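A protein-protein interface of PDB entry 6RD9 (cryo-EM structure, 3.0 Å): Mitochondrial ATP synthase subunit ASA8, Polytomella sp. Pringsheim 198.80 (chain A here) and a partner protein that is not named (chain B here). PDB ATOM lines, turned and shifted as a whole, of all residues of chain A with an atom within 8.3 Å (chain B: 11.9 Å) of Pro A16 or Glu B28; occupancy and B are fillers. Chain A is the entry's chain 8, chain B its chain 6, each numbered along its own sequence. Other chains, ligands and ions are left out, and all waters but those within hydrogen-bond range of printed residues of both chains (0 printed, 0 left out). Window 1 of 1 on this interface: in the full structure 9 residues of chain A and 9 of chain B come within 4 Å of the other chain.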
ATOM      1  N   GLU A   5     -27.822  -1.757  -9.726  1.00  0.00           N
ATOM      2  CA  GLU A   5     -27.256  -0.833  -8.738  1.00  0.00           C
ATOM      3  C   GLU A   5     -27.445   0.633  -9.083  1.00  0.00           C
ATOM      4  O   GLU A   5     -27.212   1.500  -8.245  1.00  0.00           O
ATOM      5  CB  GLU A   5     -25.770  -1.099  -8.497  1.00  0.00           C
ATOM      6  CG  GLU A   5     -25.314  -0.799  -7.108  1.00  0.00           C
ATOM      7  CD  GLU A   5     -23.848  -0.477  -7.059  1.00  0.00           C
ATOM      8  OE1 GLU A   5     -23.108  -0.966  -7.931  1.00  0.00           O
ATOM      9  OE2 GLU A   5     -23.433   0.282  -6.161  1.00  0.00           O
ATOM     10  N   LEU A  12     -31.653   1.821  -1.241  1.00  0.00           N
ATOM     11  CA  LEU A  12     -31.258   0.712  -0.395  1.00  0.00           C
ATOM     12  C   LEU A  12     -29.756   0.601  -0.435  1.00  0.00           C
ATOM     13  O   LEU A  12     -29.186   0.400  -1.504  1.00  0.00           O
ATOM     14  CB  LEU A  12     -31.862  -0.597  -0.874  1.00  0.00           C
ATOM     15  CG  LEU A  12     -33.331  -0.872  -0.670  1.00  0.00           C
ATOM     16  CD1 LEU A  12     -33.662  -1.946  -1.611  1.00  0.00           C
ATOM     17  CD2 LEU A  12     -33.558  -1.324   0.716  1.00  0.00           C
ATOM     18  N   ARG A  13     -29.117   0.715   0.711  1.00  0.00           N
ATOM     19  CA  ARG A  13     -27.690   0.506   0.796  1.00  0.00           C
ATOM     20  C   ARG A  13     -27.421  -0.662   1.721  1.00  0.00           C
ATOM     21  O   ARG A  13     -28.259  -1.026   2.534  1.00  0.00           O
ATOM     22  CB  ARG A  13     -26.994   1.744   1.282  1.00  0.00           C
ATOM     23  CG  ARG A  13     -27.439   2.970   0.583  1.00  0.00           C
ATOM     24  CD  ARG A  13     -26.455   4.042   0.757  1.00  0.00           C
ATOM     25  NE  ARG A  13     -26.865   5.240   0.063  1.00  0.00           N
ATOM     26  CZ  ARG A  13     -27.405   6.287   0.651  1.00  0.00           C
ATOM     27  NH1 ARG A  13     -27.741   7.340  -0.056  1.00  0.00           N
ATOM     28  NH2 ARG A  13     -27.593   6.285   1.942  1.00  0.00           N
ATOM     29  N   THR A  14     -26.268  -1.275   1.558  1.00  0.00           N
ATOM     30  CA  THR A  14     -25.848  -2.390   2.386  1.00  0.00           C
ATOM     31  C   THR A  14     -25.131  -1.845   3.610  1.00  0.00           C
ATOM     32  O   THR A  14     -24.882  -0.645   3.676  1.00  0.00           O
ATOM     33  CB  THR A  14     -24.957  -3.296   1.557  1.00  0.00           C
ATOM     34  OG1 THR A  14     -23.969  -2.488   0.933  1.00  0.00           O
ATOM     35  CG2 THR A  14     -25.769  -4.018   0.531  1.00  0.00           C
ATOM     36  N   PRO A  15     -24.828  -2.677   4.611  1.00  0.00           N
ATOM     37  CA  PRO A  15     -24.027  -2.211   5.734  1.00  0.00           C
ATOM     38  C   PRO A  15     -22.662  -1.739   5.289  1.00  0.00           C
ATOM     39  O   PRO A  15     -22.062  -2.346   4.393  1.00  0.00           O
ATOM     40  CB  PRO A  15     -23.911  -3.449   6.623  1.00  0.00           C
ATOM     41  CG  PRO A  15     -24.494  -4.520   5.870  1.00  0.00           C
ATOM     42  CD  PRO A  15     -25.484  -3.927   4.994  1.00  0.00           C
ATOM     43  N   PRO A  16     -22.162  -0.648   5.861  1.00  0.00           N
ATOM     44  CA  PRO A  16     -20.957  -0.024   5.322  1.00  0.00           C
ATOM     45  C   PRO A  16     -19.722  -0.860   5.564  1.00  0.00           C
ATOM     46  O   PRO A  16     -19.584  -1.530   6.582  1.00  0.00           O
ATOM     47  CB  PRO A  16     -20.891   1.307   6.071  1.00  0.00           C
ATOM     48  CG  PRO A  16     -21.703   1.123   7.249  1.00  0.00           C
ATOM     49  CD  PRO A  16     -22.778   0.185   6.899  1.00  0.00           C
ATOM     50  N   THR A  17     -18.833  -0.839   4.579  1.00  0.00           N
ATOM     51  CA  THR A  17     -17.577  -1.566   4.619  1.00  0.00           C
ATOM     52  C   THR A  17     -16.380  -0.656   4.773  1.00  0.00           C
ATOM     53  O   THR A  17     -15.372  -1.071   5.340  1.00  0.00           O
ATOM     54  CB  THR A  17     -17.399  -2.383   3.338  1.00  0.00           C
ATOM     55  OG1 THR A  17     -17.465  -1.505   2.217  1.00  0.00           O
ATOM     56  CG2 THR A  17     -18.487  -3.394   3.195  1.00  0.00           C
ATOM     57  N   GLY A  18     -16.466   0.569   4.281  1.00  0.00           N
ATOM     58  CA  GLY A  18     -15.353   1.479   4.386  1.00  0.00           C
ATOM     59  C   GLY A  18     -15.239   2.059   5.767  1.00  0.00           C
ATOM     60  O   GLY A  18     -14.309   1.736   6.507  1.00  0.00           O
ATOM     61  N   ALA A  19     -16.190   2.903   6.137  1.00  0.00           N
ATOM     62  CA  ALA A  19     -16.189   3.498   7.459  1.00  0.00           C
ATOM     63  C   ALA A  19     -17.616   3.847   7.818  1.00  0.00           C
ATOM     64  O   ALA A  19     -18.463   4.005   6.942  1.00  0.00           O
ATOM     65  CB  ALA A  19     -15.299   4.737   7.520  1.00  0.00           C
ATOM     66  N   ILE A  20     -17.871   3.952   9.111  1.00  0.00           N
ATOM     67  CA  ILE A  20     -19.205   4.302   9.593  1.00  0.00           C
ATOM     68  C   ILE A  20     -19.469   5.769   9.291  1.00  0.00           C
ATOM     69  O   ILE A  20     -18.649   6.622   9.654  1.00  0.00           O
ATOM     70  CB  ILE A  20     -19.311   4.015  11.073  1.00  0.00           C
ATOM     71  CG1 ILE A  20     -19.142   2.534  11.278  1.00  0.00           C
ATOM     72  CG2 ILE A  20     -20.640   4.399  11.590  1.00  0.00           C
ATOM     73  CD1 ILE A  20     -19.197   2.143  12.659  1.00  0.00           C
ATOM     74  N   PRO A  21     -20.564   6.110   8.633  1.00  0.00           N
ATOM     75  CA  PRO A  21     -20.769   7.483   8.188  1.00  0.00           C
ATOM     76  C   PRO A  21     -21.180   8.379   9.346  1.00  0.00           C
ATOM     77  O   PRO A  21     -21.283   7.963  10.491  1.00  0.00           O
ATOM     78  CB  PRO A  21     -21.895   7.353   7.171  1.00  0.00           C
ATOM     79  CG  PRO A  21     -22.121   5.939   7.002  1.00  0.00           C
ATOM     80  CD  PRO A  21     -21.655   5.245   8.182  1.00  0.00           C
ATOM     81  N   GLU B  28     -18.911   4.594  -1.995  1.00  0.00           N
ATOM     82  CA  GLU B  28     -18.980   3.235  -1.480  1.00  0.00           C
ATOM     83  C   GLU B  28     -20.198   2.513  -2.036  1.00  0.00           C
ATOM     84  O   GLU B  28     -21.309   2.685  -1.540  1.00  0.00           O
ATOM     85  CB  GLU B  28     -19.023   3.249   0.042  1.00  0.00           C
ATOM     86  CG  GLU B  28     -18.962   1.881   0.677  1.00  0.00           C
ATOM     87  CD  GLU B  28     -19.059   1.938   2.180  1.00  0.00           C
ATOM     88  OE1 GLU B  28     -19.437   2.996   2.712  1.00  0.00           O
ATOM     89  OE2 GLU B  28     -18.758   0.924   2.830  1.00  0.00           O
ATOM     90  N   GLY B  29     -19.989   1.721  -3.079  1.00  0.00           N
ATOM     91  CA  GLY B  29     -21.065   0.948  -3.654  1.00  0.00           C
ATOM     92  C   GLY B  29     -21.433  -0.206  -2.762  1.00  0.00           C
ATOM     93  O   GLY B  29     -20.746  -0.522  -1.793  1.00  0.00           O
ATOM     94  N   ASN B  30     -22.543  -0.853  -3.085  1.00  0.00           N
ATOM     95  CA  ASN B  30     -23.063  -1.817  -2.141  1.00  0.00           C
ATOM     96  C   ASN B  30     -22.345  -3.140  -2.281  1.00  0.00           C
ATOM     97  O   ASN B  30     -21.859  -3.492  -3.346  1.00  0.00           O
ATOM     98  CB  ASN B  30     -24.572  -1.979  -2.284  1.00  0.00           C
ATOM     99  CG  ASN B  30     -24.962  -2.799  -3.431  1.00  0.00           C
ATOM    100  OD1 ASN B  30     -24.458  -2.612  -4.504  1.00  0.00           O
ATOM    101  ND2 ASN B  30     -25.908  -3.677  -3.230  1.00  0.00           N
ATOM    102  N   SER B  31     -22.259  -3.859  -1.175  1.00  0.00           N
ATOM    103  CA  SER B  31     -21.380  -5.001  -1.074  1.00  0.00           C
ATOM    104  C   SER B  31     -21.934  -6.230  -1.742  1.00  0.00           C
ATOM    105  O   SER B  31     -21.193  -7.182  -1.952  1.00  0.00           O
ATOM    106  CB  SER B  31     -21.115  -5.326   0.376  1.00  0.00           C
ATOM    107  OG  SER B  31     -22.276  -5.827   0.980  1.00  0.00           O
ATOM    108  N   VAL B  32     -23.216  -6.255  -2.052  1.00  0.00           N
ATOM    109  CA  VAL B  32     -23.751  -7.388  -2.783  1.00  0.00           C
ATOM    110  C   VAL B  32     -23.372  -7.293  -4.248  1.00  0.00           C
ATOM    111  O   VAL B  32     -22.998  -8.290  -4.860  1.00  0.00           O
ATOM    112  CB  VAL B  32     -25.263  -7.472  -2.562  1.00  0.00           C
ATOM    113  CG1 VAL B  32     -25.834  -8.569  -3.346  1.00  0.00           C
ATOM    114  CG2 VAL B  32     -25.508  -7.749  -1.140  1.00  0.00           C
ATOM    115  N   ALA B  33     -23.396  -6.098  -4.826  1.00  0.00           N
ATOM    116  CA  ALA B  33     -22.845  -5.935  -6.161  1.00  0.00           C
ATOM    117  C   ALA B  33     -21.341  -6.120  -6.186  1.00  0.00           C
ATOM    118  O   ALA B  33     -20.782  -6.390  -7.249  1.00  0.00           O
ATOM    119  CB  ALA B  33     -23.182  -4.571  -6.729  1.00  0.00           C
ATOM    120  N   GLY B  34     -20.669  -5.966  -5.053  1.00  0.00           N
ATOM    121  CA  GLY B  34     -19.282  -6.358  -4.978  1.00  0.00           C
ATOM    122  C   GLY B  34     -19.104  -7.850  -4.863  1.00  0.00           C
ATOM    123  O   GLY B  34     -18.091  -8.383  -5.301  1.00  0.00           O
ATOM    124  N   ILE B  35     -20.063  -8.541  -4.254  1.00  0.00           N
ATOM    125  CA  ILE B  35     -20.025  -9.997  -4.199  1.00  0.00           C
ATOM    126  C   ILE B  35     -20.316 -10.573  -5.568  1.00  0.00           C
ATOM    127  O   ILE B  35     -19.627 -11.483  -6.028  1.00  0.00           O
ATOM    128  CB  ILE B  35     -21.022 -10.512  -3.147  1.00  0.00           C
ATOM    129  CG1 ILE B  35     -20.420 -10.441  -1.762  1.00  0.00           C
ATOM    130  CG2 ILE B  35     -21.427 -11.927  -3.394  1.00  0.00           C
ATOM    131  CD1 ILE B  35     -21.370 -10.821  -0.677  1.00  0.00           C
ATOM    132  N   LYS B  37     -19.925  -9.182  -8.482  1.00  0.00           N
ATOM    133  CA  LYS B  37     -18.840  -8.939  -9.420  1.00  0.00           C
ATOM    134  C   LYS B  37     -17.644  -9.824  -9.121  1.00  0.00           C
ATOM    135  O   LYS B  37     -17.077 -10.409 -10.032  1.00  0.00           O
ATOM    136  CB  LYS B  37     -18.436  -7.475  -9.404  1.00  0.00           C
ATOM    137  CG  LYS B  37     -17.984  -6.971 -10.750  1.00  0.00           C
ATOM    138  CD  LYS B  37     -17.524  -5.539 -10.694  1.00  0.00           C
ATOM    139  CE  LYS B  37     -16.311  -5.402  -9.817  1.00  0.00           C
ATOM    140  NZ  LYS B  37     -15.178  -6.214 -10.309  1.00  0.00           N
ATOM    141  N   LYS B  55     -16.093 -13.201   1.012  1.00  0.00           N
ATOM    142  CA  LYS B  55     -16.886 -13.071   2.225  1.00  0.00           C
ATOM    143  C   LYS B  55     -16.390 -11.921   3.075  1.00  0.00           C
ATOM    144  O   LYS B  55     -17.186 -11.144   3.604  1.00  0.00           O
ATOM    145  CB  LYS B  55     -16.824 -14.365   3.021  1.00  0.00           C
ATOM    146  CG  LYS B  55     -17.546 -14.366   4.323  1.00  0.00           C
ATOM    147  CD  LYS B  55     -18.994 -14.663   4.125  1.00  0.00           C
ATOM    148  CE  LYS B  55     -19.655 -14.999   5.427  1.00  0.00           C
ATOM    149  NZ  LYS B  55     -21.116 -15.168   5.253  1.00  0.00           N
ATOM    150  N   ALA B  56     -15.077 -11.791   3.207  1.00  0.00           N
ATOM    151  CA  ALA B  56     -14.483 -10.780   4.059  1.00  0.00           C
ATOM    152  C   ALA B  56     -14.323  -9.442   3.370  1.00  0.00           C
ATOM    153  O   ALA B  56     -14.093  -8.446   4.048  1.00  0.00           O
ATOM    154  CB  ALA B  56     -13.130 -11.260   4.556  1.00  0.00           C
ATOM    155  N   GLN B  57     -14.405  -9.390   2.051  1.00  0.00           N
ATOM    156  CA  GLN B  57     -14.419  -8.107   1.371  1.00  0.00           C
ATOM    157  C   GLN B  57     -15.769  -7.431   1.457  1.00  0.00           C
ATOM    158  O   GLN B  57     -15.871  -6.237   1.174  1.00  0.00           O
ATOM    159  CB  GLN B  57     -14.055  -8.278  -0.093  1.00  0.00           C
ATOM    160  CG  GLN B  57     -12.621  -8.017  -0.413  1.00  0.00           C
ATOM    161  CD  GLN B  57     -12.274  -8.407  -1.829  1.00  0.00           C
ATOM    162  OE1 GLN B  57     -13.038  -9.095  -2.498  1.00  0.00           O
ATOM    163  NE2 GLN B  57     -11.111  -7.974  -2.295  1.00  0.00           N
ATOM    164  N   ALA B  58     -16.807  -8.175   1.813  1.00  0.00           N
ATOM    165  CA  ALA B  58     -18.157  -7.654   1.913  1.00  0.00           C
ATOM    166  C   ALA B  58     -18.704  -7.746   3.320  1.00  0.00           C
ATOM    167  O   ALA B  58     -19.901  -7.547   3.518  1.00  0.00           O
ATOM    168  CB  ALA B  58     -19.081  -8.400   0.969  1.00  0.00           C
ATOM    169  N   ALA B  59     -17.869  -8.080   4.287  1.00  0.00           N
ATOM    170  CA  ALA B  59     -18.251  -7.968   5.671  1.00  0.00           C
ATOM    171  C   ALA B  59     -18.349  -6.494   6.033  1.00  0.00           C
ATOM    172  O   ALA B  59     -17.654  -5.668   5.449  1.00  0.00           O
ATOM    173  CB  ALA B  59     -17.228  -8.661   6.551  1.00  0.00           C
ATOM    174  N   PRO B  60     -19.225  -6.128   6.964  1.00  0.00           N
ATOM    175  CA  PRO B  60     -19.309  -4.728   7.363  1.00  0.00           C
ATOM    176  C   PRO B  60     -18.132  -4.338   8.231  1.00  0.00           C
ATOM    177  O   PRO B  60     -17.495  -5.170   8.872  1.00  0.00           O
ATOM    178  CB  PRO B  60     -20.615  -4.669   8.139  1.00  0.00           C
ATOM    179  CG  PRO B  60     -20.781  -5.994   8.642  1.00  0.00           C
ATOM    180  CD  PRO B  60     -20.275  -6.917   7.619  1.00  0.00           C
ATOM    181  N   ILE B  61     -17.834  -3.048   8.240  1.00  0.00           N
ATOM    182  CA  ILE B  61     -16.735  -2.559   9.058  1.00  0.00           C
ATOM    183  C   ILE B  61     -17.200  -2.489  10.501  1.00  0.00           C
ATOM    184  O   ILE B  61     -18.275  -1.973  10.805  1.00  0.00           O
ATOM    185  CB  ILE B  61     -16.208  -1.208   8.543  1.00  0.00           C
ATOM    186  CG1 ILE B  61     -15.068  -0.711   9.409  1.00  0.00           C
ATOM    187  CG2 ILE B  61     -17.267  -0.139   8.460  1.00  0.00           C
ATOM    188  CD1 ILE B  61     -13.848  -1.528   9.285  1.00  0.00           C
ATOM    189  N   TYR B  62     -16.448  -3.112  11.378  1.00  0.00           N
ATOM    190  CA  TYR B  62     -16.604  -2.905  12.805  1.00  0.00           C
ATOM    191  C   TYR B  62     -15.298  -2.300  13.248  1.00  0.00           C
ATOM    192  O   TYR B  62     -14.289  -3.026  13.311  1.00  0.00           O
ATOM    193  CB  TYR B  62     -16.865  -4.215  13.527  1.00  0.00           C
ATOM    194  CG  TYR B  62     -18.072  -4.948  13.040  1.00  0.00           C
ATOM    195  CD1 TYR B  62     -19.251  -4.296  12.809  1.00  0.00           C
ATOM    196  CD2 TYR B  62     -18.028  -6.303  12.817  1.00  0.00           C
ATOM    197  CE1 TYR B  62     -20.344  -4.965  12.373  1.00  0.00           C
ATOM    198  CE2 TYR B  62     -19.122  -6.972  12.379  1.00  0.00           C
ATOM    199  CZ  TYR B  62     -20.275  -6.295  12.163  1.00  0.00           C
ATOM    200  OH  TYR B  62     -21.373  -6.968  11.727  1.00  0.00           O
ATOM    201  N   PRO B  63     -15.255  -0.999  13.529  1.00  0.00           N
ATOM    202  CA  PRO B  63     -13.980  -0.316  13.728  1.00  0.00           C
ATOM    203  C   PRO B  63     -13.232  -0.814  14.946  1.00  0.00           C
ATOM    204  O   PRO B  63     -13.828  -1.245  15.931  1.00  0.00           O
ATOM    205  CB  PRO B  63     -14.401   1.141  13.887  1.00  0.00           C
ATOM    206  CG  PRO B  63     -15.642   1.224  13.162  1.00  0.00           C
ATOM    207  CD  PRO B  63     -16.348  -0.038  13.423  1.00  0.00           C
ATOM    208  N   ALA B  64     -11.915  -0.837  14.826  1.00  0.00           N
ATOM    209  CA  ALA B  64     -11.099  -1.514  15.808  1.00  0.00           C
ATOM    210  C   ALA B  64     -10.882  -0.628  17.020  1.00  0.00           C
ATOM    211  O   ALA B  64     -10.917   0.599  16.938  1.00  0.00           O
ATOM    212  CB  ALA B  64      -9.763  -1.922  15.202  1.00  0.00           C
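The backbone NH (N) of Ser B31 lies within hydrogen-bond range of the side-chain hydroxyl (OG1) of Thr A14, 3.0 Å away.
N of Ile B61 is in hydrogen-bond range of O of Pro A16, at 2.8 Å.
The side-chain carboxylate (OE2) of Glu B28 lies within hydrogen-bond range of the backbone NH (N) of Gly A18, at 2.7 Å.
The backbone NH (N) of Asn B30 sits at hydrogen-bond distance from the side-chain carboxylate (OE2) of Glu A5 (3.4 Å).
The side-chain carboxylate of Glu B28 sits at hydrogen-bond distance from the backbone NH of Thr A17 (2.5 Å).
Among the printed residues, merely in contact across the chains: Thr A14 with Asn B30 (3.3 Å), Pro A16 with Pro B60 (3.3 Å), Thr A17 with Ala B59 (3.3 Å), Thr A17 with Ile B61 (3.3 Å), Pro A16 with Glu B28 (3.4 Å), Glu A5 with Gly B29 (3.5 Å), Ile A20 with Pro B63 (3.7 Å), Glu A5 with Ala B33 (3.8 Å), Pro A15 with Pro B60 (3.8 Å), Gly A18 with Ile B61 (3.9 Å) and Ala A19 with Ile B61 (3.9 Å).
Printed residues of chain B within 4 Å of Glu A5: Gly B29 (3.5 Å), Asn B30 (3.3 Å) and Ala B33 (3.8 Å).
Pro A15 touches just one residue of chain B: Pro B60 (3.8 Å).
Pro A16 touches just these residues of chain B: Glu B28, Pro B60 and Ile B61.
Thr A17 touches just these residues of chain B: Glu B28, Ala B59 and Ile B61.
Gly A18 touches two residues of chain B.
No residue of chain B comes within 4 Å of Pro A21.
Glu B28 touches just these residues of chain A: Pro A16 (3.4 Å), Thr A17 (2.5 Å) and Gly A18 (2.7 Å).
Printed residues of chain A within 4 Å of Ala B33: Glu A5 (3.8 Å).
Gln B57 touches none of the printed residues of chain A.
Of the printed residues of chain A, Pro B63 touches Ile A20.
The nearest residue of chain A that does not touch Glu B28 is Ala A19 (4.5 Å).
Of the 19 printed residues of chain B, 9 touch a printed residue of chain A.
Hydrophobic or aromatic side chains of chain B that line the printed part of chain A: Ala B33, Pro B60, Ile B61 and Pro B63.
Of the 11 printed residues of chain A, 8 touch a printed residue of chain B.
Printed residues of chain A that touch a printed residue of chain B: Glu A5, Thr A14, Pro A15, Pro A16, Thr A17, Gly A18, Ala A19 and Ile A20.
Among the printed residues, no Asp or Glu carboxylate lies within 4 Å of a Lys or Arg side-chain nitrogen of the other chain.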
